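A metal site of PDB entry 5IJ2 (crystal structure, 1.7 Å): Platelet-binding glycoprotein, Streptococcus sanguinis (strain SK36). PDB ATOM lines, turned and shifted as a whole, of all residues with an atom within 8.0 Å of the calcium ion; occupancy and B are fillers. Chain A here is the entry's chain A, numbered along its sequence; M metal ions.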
ATOM      1  N   THR A   4      -5.397  -0.743   9.713  1.00  0.00           N
ATOM      2  CA  THR A   4      -6.239  -0.440   8.566  1.00  0.00           C
ATOM      3  C   THR A   4      -6.346   1.069   8.394  1.00  0.00           C
ATOM      4  O   THR A   4      -6.166   1.849   9.331  1.00  0.00           O
ATOM      5  CB  THR A   4      -7.657  -1.006   8.724  1.00  0.00           C
ATOM      6  OG1 THR A   4      -8.205  -0.570   9.968  1.00  0.00           O
ATOM      7  CG2 THR A   4      -7.663  -2.530   8.690  1.00  0.00           C
ATOM      8  N   ASP A   5      -6.648   1.452   7.160  1.00  0.00           N
ATOM      9  CA  ASP A   5      -6.932   2.821   6.765  1.00  0.00           C
ATOM     10  C   ASP A   5      -8.414   3.101   7.018  1.00  0.00           C
ATOM     11  O   ASP A   5      -9.285   2.486   6.393  1.00  0.00           O
ATOM     12  CB  ASP A   5      -6.566   2.988   5.290  1.00  0.00           C
ATOM     13  CG  ASP A   5      -6.730   4.412   4.788  1.00  0.00           C
ATOM     14  OD1 ASP A   5      -7.389   5.215   5.467  1.00  0.00           O
ATOM     15  OD2 ASP A   5      -6.225   4.737   3.685  1.00  0.00           O
ATOM     16  N   THR A   6      -8.696   4.029   7.909  1.00  0.00           N
ATOM     17  CA  THR A   6     -10.071   4.367   8.241  1.00  0.00           C
ATOM     18  C   THR A   6     -10.332   5.840   8.008  1.00  0.00           C
ATOM     19  O   THR A   6     -11.364   6.360   8.438  1.00  0.00           O
ATOM     20  CB  THR A   6     -10.393   4.017   9.690  1.00  0.00           C
ATOM     21  OG1 THR A   6      -9.557   4.798  10.540  1.00  0.00           O
ATOM     22  CG2 THR A   6     -10.145   2.523   9.984  1.00  0.00           C
ATOM     23  N   THR A   7      -9.426   6.513   7.305  1.00  0.00           N
ATOM     24  CA  THR A   7      -9.450   7.964   7.178  1.00  0.00           C
ATOM     25  C   THR A   7      -9.674   8.328   5.729  1.00  0.00           C
ATOM     26  O   THR A   7      -8.861   7.908   4.881  1.00  0.00           O
ATOM     27  CB  THR A   7      -8.127   8.548   7.653  1.00  0.00           C
ATOM     28  OG1 THR A   7      -7.893   8.117   8.996  1.00  0.00           O
ATOM     29  CG2 THR A   7      -8.182  10.099   7.606  1.00  0.00           C
ATOM     30  N   PRO A   8     -10.695   9.101   5.378  1.00  0.00           N
ATOM     31  CA  PRO A   8     -10.926   9.413   3.979  1.00  0.00           C
ATOM     32  C   PRO A   8      -9.949  10.455   3.493  1.00  0.00           C
ATOM     33  O   PRO A   8      -9.243  11.108   4.285  1.00  0.00           O
ATOM     34  CB  PRO A   8     -12.369   9.959   3.964  1.00  0.00           C
ATOM     35  CG  PRO A   8     -12.633  10.389   5.348  1.00  0.00           C
ATOM     36  CD  PRO A   8     -11.771   9.590   6.268  1.00  0.00           C
ATOM     37  N   PRO A   9      -9.912  10.654   2.180  1.00  0.00           N
ATOM     38  CA  PRO A   9      -9.063  11.689   1.591  1.00  0.00           C
ATOM     39  C   PRO A   9      -9.488  13.063   2.057  1.00  0.00           C
ATOM     40  O   PRO A   9     -10.594  13.275   2.555  1.00  0.00           O
ATOM     41  CB  PRO A   9      -9.294  11.533   0.081  1.00  0.00           C
ATOM     42  CG  PRO A   9      -9.749  10.098  -0.074  1.00  0.00           C
ATOM     43  CD  PRO A   9     -10.555   9.802   1.167  1.00  0.00           C
ATOM     44  N   THR A  10      -8.576  14.011   1.860  1.00  0.00           N
ATOM     45  CA  THR A  10      -8.788  15.412   2.184  1.00  0.00           C
ATOM     46  C   THR A  10      -8.711  16.218   0.902  1.00  0.00           C
ATOM     47  O   THR A  10      -7.729  16.104   0.143  1.00  0.00           O
ATOM     48  CB  THR A  10      -7.709  15.909   3.168  1.00  0.00           C
ATOM     49  OG1 THR A  10      -7.825  15.208   4.410  1.00  0.00           O
ATOM     50  CG2 THR A  10      -7.887  17.371   3.419  1.00  0.00           C
ATOM     51  N   THR A  32      -5.323  14.739  -1.104  1.00  0.00           N
ATOM     52  CA  THR A  32      -4.325  13.898  -0.469  1.00  0.00           C
ATOM     53  C   THR A  32      -5.046  12.807   0.320  1.00  0.00           C
ATOM     54  O   THR A  32      -6.220  12.949   0.664  1.00  0.00           O
ATOM     55  CB  THR A  32      -3.412  14.660   0.489  1.00  0.00           C
ATOM     56  OG1 THR A  32      -4.193  15.078   1.616  1.00  0.00           O
ATOM     57  CG2 THR A  32      -2.766  15.864  -0.183  1.00  0.00           C
ATOM     58  N   ASP A  33      -4.358  11.711   0.576  1.00  0.00           N
ATOM     59  CA  ASP A  33      -4.895  10.692   1.473  1.00  0.00           C
ATOM     60  C   ASP A  33      -3.741  10.164   2.310  1.00  0.00           C
ATOM     61  O   ASP A  33      -2.610  10.089   1.845  1.00  0.00           O
ATOM     62  CB  ASP A  33      -5.550   9.542   0.722  1.00  0.00           C
ATOM     63  CG  ASP A  33      -6.229   8.563   1.672  1.00  0.00           C
ATOM     64  OD1 ASP A  33      -7.232   8.954   2.284  1.00  0.00           O
ATOM     65  OD2 ASP A  33      -5.760   7.407   1.847  1.00  0.00           O
ATOM     66  N   ASP A  34      -4.058   9.759   3.555  1.00  0.00           N
ATOM     67  CA  ASP A  34      -3.001   9.248   4.417  1.00  0.00           C
ATOM     68  C   ASP A  34      -2.299   8.027   3.825  1.00  0.00           C
ATOM     69  O   ASP A  34      -1.126   7.795   4.116  1.00  0.00           O
ATOM     70  CB  ASP A  34      -3.557   8.967   5.824  1.00  0.00           C
ATOM     71  CG  ASP A  34      -4.648   7.878   5.850  1.00  0.00           C
ATOM     72  OD1 ASP A  34      -5.469   7.761   4.915  1.00  0.00           O
ATOM     73  OD2 ASP A  34      -4.709   7.149   6.870  1.00  0.00           O
ATOM     74  N   SER A  35      -2.991   7.254   2.985  1.00  0.00           N
ATOM     75  CA  SER A  35      -2.401   6.105   2.291  1.00  0.00           C
ATOM     76  C   SER A  35      -1.535   6.504   1.126  1.00  0.00           C
ATOM     77  O   SER A  35      -0.810   5.651   0.577  1.00  0.00           O
ATOM     78  CB  SER A  35      -3.486   5.194   1.737  1.00  0.00           C
ATOM     79  OG  SER A  35      -4.159   5.793   0.628  1.00  0.00           O
ATOM     80  N   GLY A  36      -1.646   7.742   0.660  1.00  0.00           N
ATOM     81  CA  GLY A  36      -1.002   8.140  -0.563  1.00  0.00           C
ATOM     82  C   GLY A  36      -1.759   7.828  -1.850  1.00  0.00           C
ATOM     83  O   GLY A  36      -1.240   8.152  -2.926  1.00  0.00           O
ATOM     84  N   GLN A  37      -2.950   7.237  -1.788  1.00  0.00           N
ATOM     85  CA  GLN A  37      -3.670   6.840  -2.993  1.00  0.00           C
ATOM     86  C   GLN A  37      -5.130   7.274  -2.939  1.00  0.00           C
ATOM     87  O   GLN A  37      -5.842   6.939  -1.986  1.00  0.00           O
ATOM     88  CB  GLN A  37      -3.621   5.317  -3.197  1.00  0.00           C
ATOM     89  CG  GLN A  37      -4.327   4.839  -4.468  1.00  0.00           C
ATOM     90  CD  GLN A  37      -4.033   3.390  -4.766  1.00  0.00           C
ATOM     91  OE1 GLN A  37      -3.098   2.808  -4.202  1.00  0.00           O
ATOM     92  NE2 GLN A  37      -4.858   2.779  -5.620  1.00  0.00           N
ATOM     93  N   VAL A  38      -5.570   7.993  -3.976  1.00  0.00           N
ATOM     94  CA  VAL A  38      -6.956   8.378  -4.137  1.00  0.00           C
ATOM     95  C   VAL A  38      -7.500   7.615  -5.343  1.00  0.00           C
ATOM     96  O   VAL A  38      -6.882   7.630  -6.416  1.00  0.00           O
ATOM     97  CB  VAL A  38      -7.120   9.901  -4.290  1.00  0.00           C
ATOM     98  CG1 VAL A  38      -8.492  10.250  -4.941  1.00  0.00           C
ATOM     99  CG2 VAL A  38      -6.994  10.520  -2.897  1.00  0.00           C
ATOM    100  N   TRP A 104     -12.865   9.082  -2.789  1.00  0.00           N
ATOM    101  CA  TRP A 104     -12.589   7.807  -2.156  1.00  0.00           C
ATOM    102  C   TRP A 104     -11.085   7.537  -2.139  1.00  0.00           C
ATOM    103  O   TRP A 104     -10.386   7.863  -3.100  1.00  0.00           O
ATOM    104  CB  TRP A 104     -13.249   6.658  -2.936  1.00  0.00           C
ATOM    105  CG  TRP A 104     -14.702   6.518  -2.817  1.00  0.00           C
ATOM    106  CD1 TRP A 104     -15.353   5.564  -2.102  1.00  0.00           C
ATOM    107  CD2 TRP A 104     -15.712   7.281  -3.493  1.00  0.00           C
ATOM    108  NE1 TRP A 104     -16.704   5.705  -2.249  1.00  0.00           N
ATOM    109  CE2 TRP A 104     -16.961   6.745  -3.107  1.00  0.00           C
ATOM    110  CE3 TRP A 104     -15.678   8.360  -4.394  1.00  0.00           C
ATOM    111  CZ2 TRP A 104     -18.175   7.265  -3.541  1.00  0.00           C
ATOM    112  CZ3 TRP A 104     -16.886   8.880  -4.849  1.00  0.00           C
ATOM    113  CH2 TRP A 104     -18.119   8.332  -4.425  1.00  0.00           C
ATOM    114  N   ASP A 105     -10.606   6.895  -1.085  1.00  0.00           N
ATOM    115  CA  ASP A 105      -9.282   6.281  -1.147  1.00  0.00           C
ATOM    116  C   ASP A 105      -9.434   4.833  -1.641  1.00  0.00           C
ATOM    117  O   ASP A 105     -10.512   4.409  -2.055  1.00  0.00           O
ATOM    118  CB  ASP A 105      -8.561   6.403   0.198  1.00  0.00           C
ATOM    119  CG  ASP A 105      -9.228   5.618   1.327  1.00  0.00           C
ATOM    120  OD1 ASP A 105     -10.084   4.751   1.053  1.00  0.00           O
ATOM    121  OD2 ASP A 105      -8.896   5.887   2.503  1.00  0.00           O
ATOM    122  N   ALA A 106      -8.342   4.054  -1.615  1.00  0.00           N
ATOM    123  CA  ALA A 106      -8.394   2.678  -2.090  1.00  0.00           C
ATOM    124  C   ALA A 106      -8.852   1.687  -1.022  1.00  0.00           C
ATOM    125  O   ALA A 106      -8.785   0.475  -1.256  1.00  0.00           O
ATOM    126  CB  ALA A 106      -7.025   2.234  -2.607  1.00  0.00           C
ATOM    127  N   ALA A 107      -9.269   2.166   0.133  1.00  0.00           N
ATOM    128  CA  ALA A 107      -9.695   1.303   1.223  1.00  0.00           C
ATOM    129  C   ALA A 107     -11.168   1.490   1.512  1.00  0.00           C
ATOM    130  O   ALA A 107     -11.638   1.053   2.565  1.00  0.00           O
ATOM    131  CB  ALA A 107      -8.864   1.580   2.477  1.00  0.00           C
ATOM    132  N   GLY A 108     -11.890   2.176   0.637  1.00  0.00           N
ATOM    133  CA  GLY A 108     -13.312   2.363   0.796  1.00  0.00           C
ATOM    134  C   GLY A 108     -13.749   3.577   1.601  1.00  0.00           C
ATOM    135  O   GLY A 108     -14.954   3.766   1.789  1.00  0.00           O
ATOM    136  N   ASN A 109     -12.821   4.371   2.114  1.00  0.00           N
ATOM    137  CA  ASN A 109     -13.199   5.573   2.839  1.00  0.00           C
ATOM    138  C   ASN A 109     -13.520   6.682   1.861  1.00  0.00           C
ATOM    139  O   ASN A 109     -12.690   7.034   1.014  1.00  0.00           O
ATOM    140  CB  ASN A 109     -12.073   5.988   3.771  1.00  0.00           C
ATOM    141  CG  ASN A 109     -11.633   4.861   4.680  1.00  0.00           C
ATOM    142  OD1 ASN A 109     -12.409   4.414   5.525  1.00  0.00           O
ATOM    143  ND2 ASN A 109     -10.408   4.379   4.496  1.00  0.00           N
ATOM    144  N   VAL A 110     -14.705   7.274   1.983  1.00  0.00           N
ATOM    145  CA  VAL A 110     -15.108   8.385   1.129  1.00  0.00           C
ATOM    146  C   VAL A 110     -15.239   9.623   2.000  1.00  0.00           C
ATOM    147  O   VAL A 110     -15.730   9.557   3.134  1.00  0.00           O
ATOM    148  CB  VAL A 110     -16.406   8.080   0.348  1.00  0.00           C
ATOM    149  CG1 VAL A 110     -17.588   7.712   1.288  1.00  0.00           C
ATOM    150  CG2 VAL A 110     -16.753   9.239  -0.563  1.00  0.00           C
HETATM  151 CA    CA M   1      -7.193   6.940   3.720  1.00  0.00          CA
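The side-chain carboxylate of Asp 105 is in hydrogen-bond range of the backbone NH of Asn 109 (3.0 Å).
The side-chain carboxylate (OD1) of Asp 105 is in hydrogen-bond range of the backbone NH (N) of Ala 107 (2.9 Å).
OD1 of Asp 105 lies within hydrogen-bond range of N of Gly 108, 3.2 Å away.
The side-chain hydroxyl (OG) of Ser 35 lies close to the side-chain carboxylate (OD2) of Asp 33 (2.6 Å).
O of Asp 5 sits at hydrogen-bond distance from ND2 of Asn 109 (2.9 Å).
Five residues have an atom within 4 Å of the calcium ion: Asp 5, Thr 7, Asp 33, Asp 34 and Asp 105.
The nearest printed residue that does not touch the calcium ion is Asn 109 (4.2 Å).
The calcium ion is bound by O of Thr 7 (2.3 Å).
The calcium ion is bound by OD1 of Asp 34, at 2.3 Å.
The calcium ion is bound by the side-chain carboxylate (OD2) of Asp 105, 2.3 Å away.
The calcium ion is bound by OD2 of Asp 33 (2.4 Å).
OD2 of Asp 5 is bound to the calcium ion (2.4 Å).
The side-chain carboxylate (OD1) of Asp 5 binds the calcium ion (2.5 Å).
The calcium ion is bound by OD1 of Asp 33, at 2.5 Å.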
